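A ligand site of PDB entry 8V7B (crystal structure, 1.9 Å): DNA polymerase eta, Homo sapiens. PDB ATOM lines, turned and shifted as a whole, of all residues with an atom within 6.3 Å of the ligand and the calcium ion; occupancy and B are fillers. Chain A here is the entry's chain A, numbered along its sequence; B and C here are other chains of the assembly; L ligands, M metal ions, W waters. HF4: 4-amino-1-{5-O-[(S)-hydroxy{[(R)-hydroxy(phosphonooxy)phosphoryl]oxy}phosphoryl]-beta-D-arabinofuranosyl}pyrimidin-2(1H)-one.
O of Val 53 lies within hydrogen-bond range of NE of Arg 58 (2.9 Å). OD1 of Asp 118 lies close to O3' of DT 8 of chain C, 2.7 Å away. The backbone carbonyl oxygen (O) of Ile 51 is in hydrogen-bond range of the guanidinium group (NE) of Arg 64. The side-chain hydroxyl (OH) of Tyr 55 lies close to the guanidinium group (NH1) of Arg 58 (3.3 Å). The side-chain hydroxyl (OG) of Ser 116 sits close to the backbone NH (N) of Asp 118 (3.2 Å). OP1 of DT 8 of chain C is in salt-bridge range of NZ of Lys 227. The backbone carbonyl oxygen (O) of Asp 16 lies within hydrogen-bond range of the side-chain amino group (NZ) of Lys 234, 3.5 Å away. O3' of DT 8 of chain C sits at hydrogen-bond distance from OG of Ser 116 (2.7 Å).
An oxygen (O1G) of the ligand lies within hydrogen-bond range of the backbone NH of Cys 19, at 3.0 Å. O of Ile 51 lies within hydrogen-bond range of O2' of the ligand (2.5 Å). NZ of Lys 234 is in salt-bridge range of O1G of the ligand. O6 of DG 4 of chain B is in hydrogen-bond range of N4 of the ligand (3.0 Å). The guanidinium group (NH1) of Arg 58 lies within salt-bridge range of an oxygen (O2G) of the ligand. The backbone NH (N) of Phe 21 is in hydrogen-bond range of an oxygen (O3') of the ligand (3.1 Å). An oxygen (O1B) of the ligand lies within salt-bridge range of the guanidinium group of Arg 64 (3.5 Å). O1G of the ligand is in hydrogen-bond range of OH of Tyr 55 (2.6 Å). O3' of the ligand sits at hydrogen-bond distance from N of Phe 20.
Asp 18 touches the ligand (CA to O1G, 3.4 Å). Ala 52 touches the ligand. Ile 117 touches the ligand. N1 of DA 5 of chain B touches N3 of the ligand, 3.9 Å away. DT 8 of chain C touches the ligand (C2' to O5', 3.2 Å). Hydrophobic or aromatic side chains within 4 Å of the ligand: Phe 20, Phe 21, Ala 52, Tyr 55 and Ile 117. 17 residues have an atom within 4 Å of the ligand: Asp 16, Met 17, Asp 18, Cys 19, Phe 20, Phe 21, Ile 51, Ala 52, Tyr 55, Arg 58, Arg 64, Ile 117, Asp 118, Lys 234, DG 4 of chain B, DA 5 of chain B and DT 8 of chain C. The nearest printed residue that does not touch the ligand is DT 3 of chain B (4.4 Å).
Within 4 Å of the calcium ion: Asp 16, Met 17 and Asp 118. Along chain A the residues within 4 Å of the calcium ion span positions 16 to 118.
O of Met 17 binds the calcium ion. The calcium ion is bound by OD2 of Asp 16, 2.3 Å away. OD2 of Asp 118 is bound to the calcium ion, 2.3 Å away. The calcium ion is bound by an oxygen (O2B) of the ligand, 2.3 Å away. An oxygen (O3G) of the ligand binds the calcium ion. The calcium ion is bound by O2A of the ligand (2.4 Å). OD1 of Asp 16 binds the calcium ion (2.7 Å). The calcium ion has seven donor atoms within binding distance.
Water W6 lies within hydrogen-bond range of an oxygen (O1A) of the ligand (2.6 Å) and the guanidinium group (NH1) of Arg 64 (2.7 Å). Water W1 lies within hydrogen-bond range of an oxygen (O1A) of the ligand (2.8 Å) and OP2 of DT 8 of chain C (3.2 Å). Water W4 lies within hydrogen-bond range of O2 of DT 8 of chain C (2.5 Å) and O4' of the ligand (2.9 Å).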
ATOM      1  N   ASP A  16      -8.564 -20.635  25.614  1.00  0.00           N
ATOM      2  CA  ASP A  16      -7.210 -20.647  26.197  1.00  0.00           C
ATOM      3  C   ASP A  16      -7.276 -20.003  27.584  1.00  0.00           C
ATOM      4  O   ASP A  16      -7.689 -18.859  27.739  1.00  0.00           O
ATOM      5  CB  ASP A  16      -6.223 -19.841  25.359  1.00  0.00           C
ATOM      6  CG  ASP A  16      -4.860 -19.765  26.041  1.00  0.00           C
ATOM      7  OD1 ASP A  16      -4.136 -20.747  25.975  1.00  0.00           O
ATOM      8  OD2 ASP A  16      -4.578 -18.735  26.646  1.00  0.00           O
ATOM      9  N   MET A  17      -6.801 -20.744  28.580  1.00  0.00           N
ATOM     10  CA  MET A  17      -6.810 -20.245  29.962  1.00  0.00           C
ATOM     11  C   MET A  17      -5.825 -19.073  30.110  1.00  0.00           C
ATOM     12  O   MET A  17      -4.752 -19.137  29.540  1.00  0.00           O
ATOM     13  CB  MET A  17      -6.462 -21.362  30.947  1.00  0.00           C
ATOM     14  CG  MET A  17      -7.255 -22.634  30.738  1.00  0.00           C
ATOM     15  SD  MET A  17      -9.034 -22.385  30.785  1.00  0.00           S
ATOM     16  CE  MET A  17      -9.228 -21.600  32.380  1.00  0.00           C
ATOM     17  N   ASP A  18      -6.214 -18.055  30.874  1.00  0.00           N
ATOM     18  CA  ASP A  18      -5.324 -16.901  31.141  1.00  0.00           C
ATOM     19  C   ASP A  18      -4.278 -17.276  32.197  1.00  0.00           C
ATOM     20  O   ASP A  18      -4.677 -17.821  33.224  1.00  0.00           O
ATOM     21  CB  ASP A  18      -6.154 -15.693  31.574  1.00  0.00           C
ATOM     22  CG  ASP A  18      -7.205 -15.250  30.556  1.00  0.00           C
ATOM     23  OD1 ASP A  18      -6.932 -15.330  29.360  1.00  0.00           O
ATOM     24  OD2 ASP A  18      -8.282 -14.824  30.984  1.00  0.00           O
ATOM     25  N   CYS A  19      -3.008 -16.935  31.972  1.00  0.00           N
ATOM     26  CA  CYS A  19      -1.901 -17.230  32.936  1.00  0.00           C
ATOM     27  C   CYS A  19      -2.215 -18.531  33.710  1.00  0.00           C
ATOM     28  O   CYS A  19      -2.301 -18.466  34.924  1.00  0.00           O
ATOM     29  CB  CYS A  19      -1.618 -15.998  33.794  1.00  0.00           C
ATOM     30  SG  CYS A  19      -3.040 -15.289  34.646  1.00  0.00           S
ATOM     31  N   PHE A  20      -2.367 -19.620  32.978  1.00  0.00           N
ATOM     32  CA  PHE A  20      -2.899 -20.861  33.587  1.00  0.00           C
ATOM     33  C   PHE A  20      -2.192 -21.235  34.884  1.00  0.00           C
ATOM     34  O   PHE A  20      -2.852 -21.279  35.916  1.00  0.00           O
ATOM     35  CB  PHE A  20      -2.892 -22.008  32.577  1.00  0.00           C
ATOM     36  CG  PHE A  20      -3.634 -23.223  33.059  1.00  0.00           C
ATOM     37  CD1 PHE A  20      -4.884 -23.086  33.647  1.00  0.00           C
ATOM     38  CD2 PHE A  20      -3.078 -24.486  32.952  1.00  0.00           C
ATOM     39  CE1 PHE A  20      -5.564 -24.205  34.098  1.00  0.00           C
ATOM     40  CE2 PHE A  20      -3.767 -25.600  33.404  1.00  0.00           C
ATOM     41  CZ  PHE A  20      -5.011 -25.454  33.983  1.00  0.00           C
ATOM     42  N   PHE A  21      -0.898 -21.532  34.802  1.00  0.00           N
ATOM     43  CA  PHE A  21      -0.201 -22.019  36.027  1.00  0.00           C
ATOM     44  C   PHE A  21      -0.409 -21.002  37.153  1.00  0.00           C
ATOM     45  O   PHE A  21      -0.614 -21.415  38.295  1.00  0.00           O
ATOM     46  CB  PHE A  21       1.257 -22.351  35.749  1.00  0.00           C
ATOM     47  CG  PHE A  21       1.498 -23.562  34.873  1.00  0.00           C
ATOM     48  CD1 PHE A  21       0.464 -24.139  34.156  1.00  0.00           C
ATOM     49  CD2 PHE A  21       2.760 -24.104  34.774  1.00  0.00           C
ATOM     50  CE1 PHE A  21       0.702 -25.241  33.353  1.00  0.00           C
ATOM     51  CE2 PHE A  21       2.993 -25.215  33.969  1.00  0.00           C
ATOM     52  CZ  PHE A  21       1.955 -25.779  33.264  1.00  0.00           C
ATOM     53  N   VAL A  22      -0.383 -19.695  36.843  1.00  0.00           N
ATOM     54  CA  VAL A  22      -0.596 -18.677  37.869  1.00  0.00           C
ATOM     55  C   VAL A  22      -1.996 -18.815  38.477  1.00  0.00           C
ATOM     56  O   VAL A  22      -2.163 -18.774  39.699  1.00  0.00           O
ATOM     57  CB  VAL A  22      -0.357 -17.266  37.308  1.00  0.00           C
ATOM     58  CG1 VAL A  22      -0.855 -16.222  38.287  1.00  0.00           C
ATOM     59  CG2 VAL A  22       1.146 -17.032  36.981  1.00  0.00           C
ATOM     60  N   ILE A  51       8.226 -19.430  34.860  1.00  0.00           N
ATOM     61  CA  ILE A  51       7.553 -20.121  33.769  1.00  0.00           C
ATOM     62  C   ILE A  51       6.150 -19.585  33.485  1.00  0.00           C
ATOM     63  O   ILE A  51       5.601 -19.889  32.426  1.00  0.00           O
ATOM     64  CB  ILE A  51       7.504 -21.646  33.986  1.00  0.00           C
ATOM     65  CG1 ILE A  51       6.687 -22.060  35.208  1.00  0.00           C
ATOM     66  CG2 ILE A  51       8.946 -22.201  34.147  1.00  0.00           C
ATOM     67  CD1 ILE A  51       6.509 -23.555  35.277  1.00  0.00           C
ATOM     68  N   ALA A  52       5.547 -18.784  34.377  1.00  0.00           N
ATOM     69  CA  ALA A  52       4.238 -18.164  34.113  1.00  0.00           C
ATOM     70  C   ALA A  52       4.107 -16.868  34.907  1.00  0.00           C
ATOM     71  O   ALA A  52       4.671 -16.771  35.994  1.00  0.00           O
ATOM     72  CB  ALA A  52       3.086 -19.114  34.472  1.00  0.00           C
ATOM     73  N   VAL A  53       3.334 -15.911  34.398  1.00  0.00           N
ATOM     74  CA  VAL A  53       3.335 -14.529  34.900  1.00  0.00           C
ATOM     75  C   VAL A  53       1.927 -13.954  34.912  1.00  0.00           C
ATOM     76  O   VAL A  53       1.237 -13.975  33.884  1.00  0.00           O
ATOM     77  CB  VAL A  53       4.255 -13.637  34.042  1.00  0.00           C
ATOM     78  CG1 VAL A  53       4.387 -12.234  34.627  1.00  0.00           C
ATOM     79  CG2 VAL A  53       5.644 -14.237  33.936  1.00  0.00           C
ATOM     80  N   TYR A  55      -0.988 -11.069  34.924  1.00  0.00           N
ATOM     81  CA  TYR A  55      -1.076  -9.851  34.111  1.00  0.00           C
ATOM     82  C   TYR A  55      -0.601  -8.614  34.889  1.00  0.00           C
ATOM     83  O   TYR A  55       0.030  -7.697  34.325  1.00  0.00           O
ATOM     84  CB  TYR A  55      -2.513  -9.686  33.596  1.00  0.00           C
ATOM     85  CG  TYR A  55      -2.748 -10.584  32.381  1.00  0.00           C
ATOM     86  CD1 TYR A  55      -3.022 -11.931  32.537  1.00  0.00           C
ATOM     87  CD2 TYR A  55      -2.607 -10.085  31.098  1.00  0.00           C
ATOM     88  CE1 TYR A  55      -3.187 -12.775  31.419  1.00  0.00           C
ATOM     89  CE2 TYR A  55      -2.762 -10.890  29.984  1.00  0.00           C
ATOM     90  CZ  TYR A  55      -3.063 -12.245  30.139  1.00  0.00           C
ATOM     91  OH  TYR A  55      -3.218 -13.048  29.015  1.00  0.00           O
ATOM     92  N   ARG A  58       3.098  -8.744  34.493  1.00  0.00           N
ATOM     93  CA  ARG A  58       3.515  -8.379  33.135  1.00  0.00           C
ATOM     94  C   ARG A  58       3.590  -6.872  32.947  1.00  0.00           C
ATOM     95  O   ARG A  58       4.412  -6.392  32.154  1.00  0.00           O
ATOM     96  CB  ARG A  58       2.573  -8.961  32.096  1.00  0.00           C
ATOM     97  CG  ARG A  58       2.488 -10.468  32.123  1.00  0.00           C
ATOM     98  CD  ARG A  58       1.420 -10.977  31.162  1.00  0.00           C
ATOM     99  NE  ARG A  58       1.184 -12.394  31.451  1.00  0.00           N
ATOM    100  CZ  ARG A  58       0.559 -13.234  30.635  1.00  0.00           C
ATOM    101  NH1 ARG A  58       0.078 -12.838  29.461  1.00  0.00           N
ATOM    102  NH2 ARG A  58       0.428 -14.511  31.009  1.00  0.00           N
ATOM    103  N   ARG A  64       8.226 -14.815  31.007  1.00  0.00           N
ATOM    104  CA  ARG A  64       8.729 -16.173  31.091  1.00  0.00           C
ATOM    105  C   ARG A  64      10.212 -16.219  30.693  1.00  0.00           C
ATOM    106  O   ARG A  64      10.685 -15.396  29.898  1.00  0.00           O
ATOM    107  CB  ARG A  64       7.882 -17.074  30.178  1.00  0.00           C
ATOM    108  CG  ARG A  64       8.351 -18.481  29.934  1.00  0.00           C
ATOM    109  CD  ARG A  64       7.308 -19.162  29.065  1.00  0.00           C
ATOM    110  NE  ARG A  64       5.999 -19.264  29.718  1.00  0.00           N
ATOM    111  CZ  ARG A  64       4.872 -18.862  29.148  1.00  0.00           C
ATOM    112  NH1 ARG A  64       4.860 -18.278  27.964  1.00  0.00           N
ATOM    113  NH2 ARG A  64       3.723 -19.007  29.806  1.00  0.00           N
ATOM    114  N   LEU A  92       4.757 -31.492  37.310  1.00  0.00           N
ATOM    115  CA  LEU A  92       3.676 -30.641  36.819  1.00  0.00           C
ATOM    116  C   LEU A  92       2.292 -31.234  37.087  1.00  0.00           C
ATOM    117  O   LEU A  92       1.331 -30.815  36.458  1.00  0.00           O
ATOM    118  CB  LEU A  92       3.864 -30.366  35.330  1.00  0.00           C
ATOM    119  CG  LEU A  92       5.251 -29.800  34.980  1.00  0.00           C
ATOM    120  CD1 LEU A  92       5.435 -29.636  33.479  1.00  0.00           C
ATOM    121  CD2 LEU A  92       5.434 -28.487  35.706  1.00  0.00           C
ATOM    122  N   SER A 116      -3.240 -28.317  23.985  1.00  0.00           N
ATOM    123  CA  SER A 116      -2.141 -28.150  24.969  1.00  0.00           C
ATOM    124  C   SER A 116      -2.696 -28.295  26.391  1.00  0.00           C
ATOM    125  O   SER A 116      -3.882 -28.514  26.538  1.00  0.00           O
ATOM    126  CB  SER A 116      -1.513 -26.803  24.803  1.00  0.00           C
ATOM    127  OG  SER A 116      -2.337 -25.782  25.337  1.00  0.00           O
ATOM    128  N   ILE A 117      -1.825 -28.129  27.385  1.00  0.00           N
ATOM    129  CA  ILE A 117      -2.251 -28.185  28.807  1.00  0.00           C
ATOM    130  C   ILE A 117      -3.395 -27.198  29.076  1.00  0.00           C
ATOM    131  O   ILE A 117      -4.204 -27.476  29.951  1.00  0.00           O
ATOM    132  CB  ILE A 117      -1.062 -27.890  29.735  1.00  0.00           C
ATOM    133  CG1 ILE A 117      -1.417 -28.195  31.190  1.00  0.00           C
ATOM    134  CG2 ILE A 117      -0.583 -26.459  29.559  1.00  0.00           C
ATOM    135  CD1 ILE A 117      -0.339 -28.934  31.935  1.00  0.00           C
ATOM    136  N   ASP A 118      -3.474 -26.095  28.320  1.00  0.00           N
ATOM    137  CA  ASP A 118      -4.481 -25.056  28.675  1.00  0.00           C
ATOM    138  C   ASP A 118      -5.271 -24.531  27.464  1.00  0.00           C
ATOM    139  O   ASP A 118      -5.893 -23.474  27.589  1.00  0.00           O
ATOM    140  CB  ASP A 118      -3.804 -23.905  29.424  1.00  0.00           C
ATOM    141  CG  ASP A 118      -3.214 -22.857  28.502  1.00  0.00           C
ATOM    142  OD1 ASP A 118      -2.671 -23.253  27.463  1.00  0.00           O
ATOM    143  OD2 ASP A 118      -3.320 -21.673  28.832  1.00  0.00           O
ATOM    144  N   GLU A 119      -5.229 -25.250  26.360  1.00  0.00           N
ATOM    145  CA  GLU A 119      -5.969 -24.823  25.159  1.00  0.00           C
ATOM    146  C   GLU A 119      -6.753 -25.974  24.531  1.00  0.00           C
ATOM    147  O   GLU A 119      -6.235 -27.083  24.471  1.00  0.00           O
ATOM    148  CB  GLU A 119      -5.044 -24.310  24.058  1.00  0.00           C
ATOM    149  CG  GLU A 119      -4.218 -23.123  24.459  1.00  0.00           C
ATOM    150  CD  GLU A 119      -3.458 -22.565  23.262  1.00  0.00           C
ATOM    151  OE1 GLU A 119      -3.406 -23.252  22.232  1.00  0.00           O
ATOM    152  OE2 GLU A 119      -2.924 -21.461  23.382  1.00  0.00           O
ATOM    153  N   LYS A 227      -7.581 -19.074  16.802  1.00  0.00           N
ATOM    154  CA  LYS A 227      -6.403 -18.832  17.643  1.00  0.00           C
ATOM    155  C   LYS A 227      -5.967 -17.367  17.581  1.00  0.00           C
ATOM    156  O   LYS A 227      -5.712 -16.725  18.616  1.00  0.00           O
ATOM    157  CB  LYS A 227      -5.262 -19.760  17.170  1.00  0.00           C
ATOM    158  CG  LYS A 227      -3.872 -19.571  17.834  1.00  0.00           C
ATOM    159  CD  LYS A 227      -3.949 -19.748  19.324  1.00  0.00           C
ATOM    160  CE  LYS A 227      -2.553 -19.815  19.981  1.00  0.00           C
ATOM    161  NZ  LYS A 227      -2.741 -19.757  21.466  1.00  0.00           N
ATOM    162  N   LYS A 234      -7.147 -10.161  25.426  1.00  0.00           N
ATOM    163  CA  LYS A 234      -6.852 -10.937  26.609  1.00  0.00           C
ATOM    164  C   LYS A 234      -6.592  -9.963  27.741  1.00  0.00           C
ATOM    165  O   LYS A 234      -6.214  -8.812  27.484  1.00  0.00           O
ATOM    166  CB  LYS A 234      -5.618 -11.830  26.401  1.00  0.00           C
ATOM    167  CG  LYS A 234      -5.834 -13.190  25.740  1.00  0.00           C
ATOM    168  CD  LYS A 234      -4.614 -14.115  25.992  1.00  0.00           C
ATOM    169  CE  LYS A 234      -4.936 -15.632  25.948  1.00  0.00           C
ATOM    170  NZ  LYS A 234      -5.410 -16.305  27.263  1.00  0.00           N
ATOM    171  N   PRO A 235      -6.813 -10.356  28.996  1.00  0.00           N
ATOM    172  CA  PRO A 235      -7.404 -11.608  29.473  1.00  0.00           C
ATOM    173  C   PRO A 235      -8.922 -11.537  29.611  1.00  0.00           C
ATOM    174  O   PRO A 235      -9.500 -10.453  29.468  1.00  0.00           O
ATOM    175  CB  PRO A 235      -6.778 -11.761  30.845  1.00  0.00           C
ATOM    176  CG  PRO A 235      -6.662 -10.315  31.334  1.00  0.00           C
ATOM    177  CD  PRO A 235      -6.351  -9.492  30.106  1.00  0.00           C
ATOM    178  P    DT B   3      20.621 -19.528  29.751  1.00  0.00           P
ATOM    179  OP1  DT B   3      21.797 -19.555  28.843  1.00  0.00           O
ATOM    180  OP2  DT B   3      20.054 -18.241  30.223  1.00  0.00           O
ATOM    181  O5'  DT B   3      19.460 -20.356  29.037  1.00  0.00           O
ATOM    182  C5'  DT B   3      18.105 -20.138  29.413  1.00  0.00           C
ATOM    183  C4'  DT B   3      17.699 -21.098  30.495  1.00  0.00           C
ATOM    184  O4'  DT B   3      16.353 -20.789  30.941  1.00  0.00           O
ATOM    185  C3'  DT B   3      17.659 -22.557  30.055  1.00  0.00           C
ATOM    186  O3'  DT B   3      18.072 -23.397  31.121  1.00  0.00           O
ATOM    187  C2'  DT B   3      16.194 -22.772  29.700  1.00  0.00           C
ATOM    188  C1'  DT B   3      15.487 -21.905  30.729  1.00  0.00           C
ATOM    189  N1   DT B   3      14.177 -21.385  30.222  1.00  0.00           N
ATOM    190  C2   DT B   3      13.093 -21.267  31.080  1.00  0.00           C
ATOM    191  O2   DT B   3      13.126 -21.565  32.275  1.00  0.00           O
ATOM    192  N3   DT B   3      11.956 -20.776  30.480  1.00  0.00           N
ATOM    193  C4   DT B   3      11.804 -20.408  29.142  1.00  0.00           C
ATOM    194  O4   DT B   3      10.751 -19.968  28.696  1.00  0.00           O
ATOM    195  C5   DT B   3      12.990 -20.551  28.311  1.00  0.00           C
ATOM    196  C7   DT B   3      12.958 -20.180  26.853  1.00  0.00           C
ATOM    197  C6   DT B   3      14.096 -21.033  28.883  1.00  0.00           C
ATOM    198  P    DG B   4      17.757 -24.961  31.051  1.00  0.00           P
ATOM    199  OP1  DG B   4      18.658 -25.668  31.990  1.00  0.00           O
ATOM    200  OP2  DG B   4      17.694 -25.335  29.622  1.00  0.00           O
ATOM    201  O5'  DG B   4      16.260 -25.061  31.593  1.00  0.00           O
ATOM    202  C5'  DG B   4      15.996 -24.986  32.990  1.00  0.00           C
ATOM    203  C4'  DG B   4      14.751 -25.789  33.315  1.00  0.00           C
ATOM    204  O4'  DG B   4      13.600 -25.193  32.665  1.00  0.00           O
ATOM    205  C3'  DG B   4      14.792 -27.240  32.815  1.00  0.00           C
ATOM    206  O3'  DG B   4      14.102 -28.012  33.726  1.00  0.00           O
ATOM    207  C2'  DG B   4      14.069 -27.162  31.465  1.00  0.00           C
ATOM    208  C1'  DG B   4      13.017 -26.114  31.760  1.00  0.00           C
ATOM    209  N9   DG B   4      12.524 -25.348  30.616  1.00  0.00           N
ATOM    210  C8   DG B   4      13.228 -24.886  29.530  1.00  0.00           C
ATOM    211  N7   DG B   4      12.487 -24.188  28.700  1.00  0.00           N
ATOM    212  C5   DG B   4      11.237 -24.179  29.305  1.00  0.00           C
ATOM    213  C6   DG B   4      10.016 -23.569  28.888  1.00  0.00           C
ATOM    214  O6   DG B   4       9.811 -22.896  27.865  1.00  0.00           O
ATOM    215  N1   DG B   4       8.980 -23.828  29.805  1.00  0.00           N
ATOM    216  C2   DG B   4       9.121 -24.551  30.974  1.00  0.00           C
ATOM    217  N2   DG B   4       8.022 -24.701  31.742  1.00  0.00           N
ATOM    218  N3   DG B   4      10.254 -25.108  31.356  1.00  0.00           N
ATOM    219  C4   DG B   4      11.254 -24.879  30.476  1.00  0.00           C
ATOM    220  P    DA B   5      13.928 -29.593  33.504  1.00  0.00           P
ATOM    221  OP1  DA B   5      14.023 -30.151  34.872  1.00  0.00           O
ATOM    222  OP2  DA B   5      14.759 -30.058  32.367  1.00  0.00           O
ATOM    223  O5'  DA B   5      12.394 -29.738  33.066  1.00  0.00           O
ATOM    224  C5'  DA B   5      11.360 -29.391  33.999  1.00  0.00           C
ATOM    225  C4'  DA B   5       9.994 -29.671  33.415  1.00  0.00           C
ATOM    226  O4'  DA B   5       9.696 -28.669  32.387  1.00  0.00           O
ATOM    227  C3'  DA B   5       9.858 -31.051  32.742  1.00  0.00           C
ATOM    228  O3'  DA B   5       8.553 -31.580  32.976  1.00  0.00           O
ATOM    229  C2'  DA B   5      10.050 -30.686  31.262  1.00  0.00           C
ATOM    230  C1'  DA B   5       9.336 -29.339  31.198  1.00  0.00           C
ATOM    231  N9   DA B   5       9.722 -28.531  30.038  1.00  0.00           N
ATOM    232  C8   DA B   5      10.959 -28.443  29.455  1.00  0.00           C
ATOM    233  N7   DA B   5      10.995 -27.658  28.393  1.00  0.00           N
ATOM    234  C5   DA B   5       9.683 -27.224  28.259  1.00  0.00           C
ATOM    235  C6   DA B   5       9.043 -26.375  27.325  1.00  0.00           C
ATOM    236  N6   DA B   5       9.679 -25.813  26.300  1.00  0.00           N
ATOM    237  N1   DA B   5       7.723 -26.152  27.480  1.00  0.00           N
ATOM    238  C2   DA B   5       7.077 -26.731  28.494  1.00  0.00           C
ATOM    239  N3   DA B   5       7.562 -27.551  29.431  1.00  0.00           N
ATOM    240  C4   DA B   5       8.878 -27.758  29.257  1.00  0.00           C
ATOM    241  P    DT C   8       1.857 -21.232  21.336  1.00  0.00           P
ATOM    242  OP1  DT C   8       0.612 -20.375  21.308  1.00  0.00           O
ATOM    243  OP2  DT C   8       3.130 -20.464  21.611  1.00  0.00           O
ATOM    244  O5'  DT C   8       1.694 -22.284  22.549  1.00  0.00           O
ATOM    245  C5'  DT C   8       0.569 -23.187  22.551  1.00  0.00           C
ATOM    246  C4'  DT C   8       0.594 -24.006  23.820  1.00  0.00           C
ATOM    247  O4'  DT C   8       1.866 -24.659  23.951  1.00  0.00           O
ATOM    248  C3'  DT C   8       0.364 -23.213  25.103  1.00  0.00           C
ATOM    249  O3'  DT C   8      -0.477 -23.945  25.989  1.00  0.00           O
ATOM    250  C2'  DT C   8       1.764 -23.077  25.672  1.00  0.00           C
ATOM    251  C1'  DT C   8       2.434 -24.367  25.230  1.00  0.00           C
ATOM    252  N1   DT C   8       3.891 -24.297  25.056  1.00  0.00           N
ATOM    253  C2   DT C   8       4.694 -24.990  25.947  1.00  0.00           C
ATOM    254  O2   DT C   8       4.241 -25.665  26.859  1.00  0.00           O
ATOM    255  N3   DT C   8       6.032 -24.881  25.717  1.00  0.00           N
ATOM    256  C4   DT C   8       6.652 -24.163  24.709  1.00  0.00           C
ATOM    257  O4   DT C   8       7.874 -24.156  24.629  1.00  0.00           O
ATOM    258  C5   DT C   8       5.756 -23.452  23.821  1.00  0.00           C
ATOM    259  C7   DT C   8       6.353 -22.641  22.712  1.00  0.00           C
ATOM    260  C6   DT C   8       4.437 -23.547  24.042  1.00  0.00           C
HETATM  261  C6  HF4 L   1       3.752 -22.276  28.425  1.00  0.00           C
HETATM  262  N4  HF4 L   1       7.112 -21.854  27.234  1.00  0.00           N
HETATM  263  C5  HF4 L   1       4.776 -21.885  27.632  1.00  0.00           C
HETATM  264  C2  HF4 L   1       5.306 -23.290  29.914  1.00  0.00           C
HETATM  265  O3G HF4 L   1      -2.251 -17.344  27.743  1.00  0.00           O
HETATM  266  PG  HF4 L   1      -1.673 -16.238  28.568  1.00  0.00           P
HETATM  267  O1G HF4 L   1      -2.729 -15.540  29.348  1.00  0.00           O
HETATM  268  O2G HF4 L   1      -0.978 -15.255  27.709  1.00  0.00           O
HETATM  269  O3B HF4 L   1      -0.589 -16.880  29.665  1.00  0.00           O
HETATM  270  PB  HF4 L   1      -0.249 -18.416  29.790  1.00  0.00           P
HETATM  271  O1B HF4 L   1       0.519 -18.590  31.048  1.00  0.00           O
HETATM  272  O2B HF4 L   1      -1.491 -19.226  29.852  1.00  0.00           O
HETATM  273  O3A HF4 L   1       0.656 -18.797  28.551  1.00  0.00           O
HETATM  274  PA  HF4 L   1       0.467 -20.009  27.564  1.00  0.00           P
HETATM  275  O1A HF4 L   1       1.391 -19.844  26.395  1.00  0.00           O
HETATM  276  O2A HF4 L   1      -0.937 -20.040  27.098  1.00  0.00           O
HETATM  277  O5' HF4 L   1       0.842 -21.425  28.306  1.00  0.00           O
HETATM  278  C5' HF4 L   1      -0.069 -21.994  29.209  1.00  0.00           C
HETATM  279  C4' HF4 L   1       0.693 -22.638  30.286  1.00  0.00           C
HETATM  280  C3' HF4 L   1       1.438 -21.576  31.076  1.00  0.00           C
HETATM  281  O3' HF4 L   1       0.632 -21.062  32.168  1.00  0.00           O
HETATM  282  C2' HF4 L   1       2.638 -22.383  31.622  1.00  0.00           C
HETATM  283  O2' HF4 L   1       3.757 -21.532  31.815  1.00  0.00           O
HETATM  284  O4' HF4 L   1       1.692 -23.524  29.727  1.00  0.00           O
HETATM  285  C1' HF4 L   1       2.904 -23.416  30.463  1.00  0.00           C
HETATM  286  N1  HF4 L   1       3.988 -22.969  29.576  1.00  0.00           N
HETATM  287  C4  HF4 L   1       6.103 -22.215  27.999  1.00  0.00           C
HETATM  288  N3  HF4 L   1       6.330 -22.900  29.121  1.00  0.00           N
HETATM  289  O2  HF4 L   1       5.540 -23.912  30.943  1.00  0.00           O
HETATM  290 CA    CA M   1      -3.028 -19.506  28.132  1.00  0.00          CA
HETATM  291  O   HOH W   1       3.665 -20.211  24.797  1.00  0.00           O
HETATM  292  O   HOH W   2      -0.957 -16.286  24.921  1.00  0.00           O
HETATM  293  O   HOH W   3       2.398 -16.634  31.885  1.00  0.00           O
HETATM  294  O   HOH W   4       2.681 -26.132  28.780  1.00  0.00           O
HETATM  295  O   HOH W   5       6.451 -19.774  25.126  1.00  0.00           O
HETATM  296  O   HOH W   6       2.751 -17.586  26.470  1.00  0.00           O
HETATM  297  O   HOH W   7       5.319 -26.522  31.765  1.00  0.00           O
HETATM  298  O   HOH W   8       1.737 -15.262  27.517  1.00  0.00           O
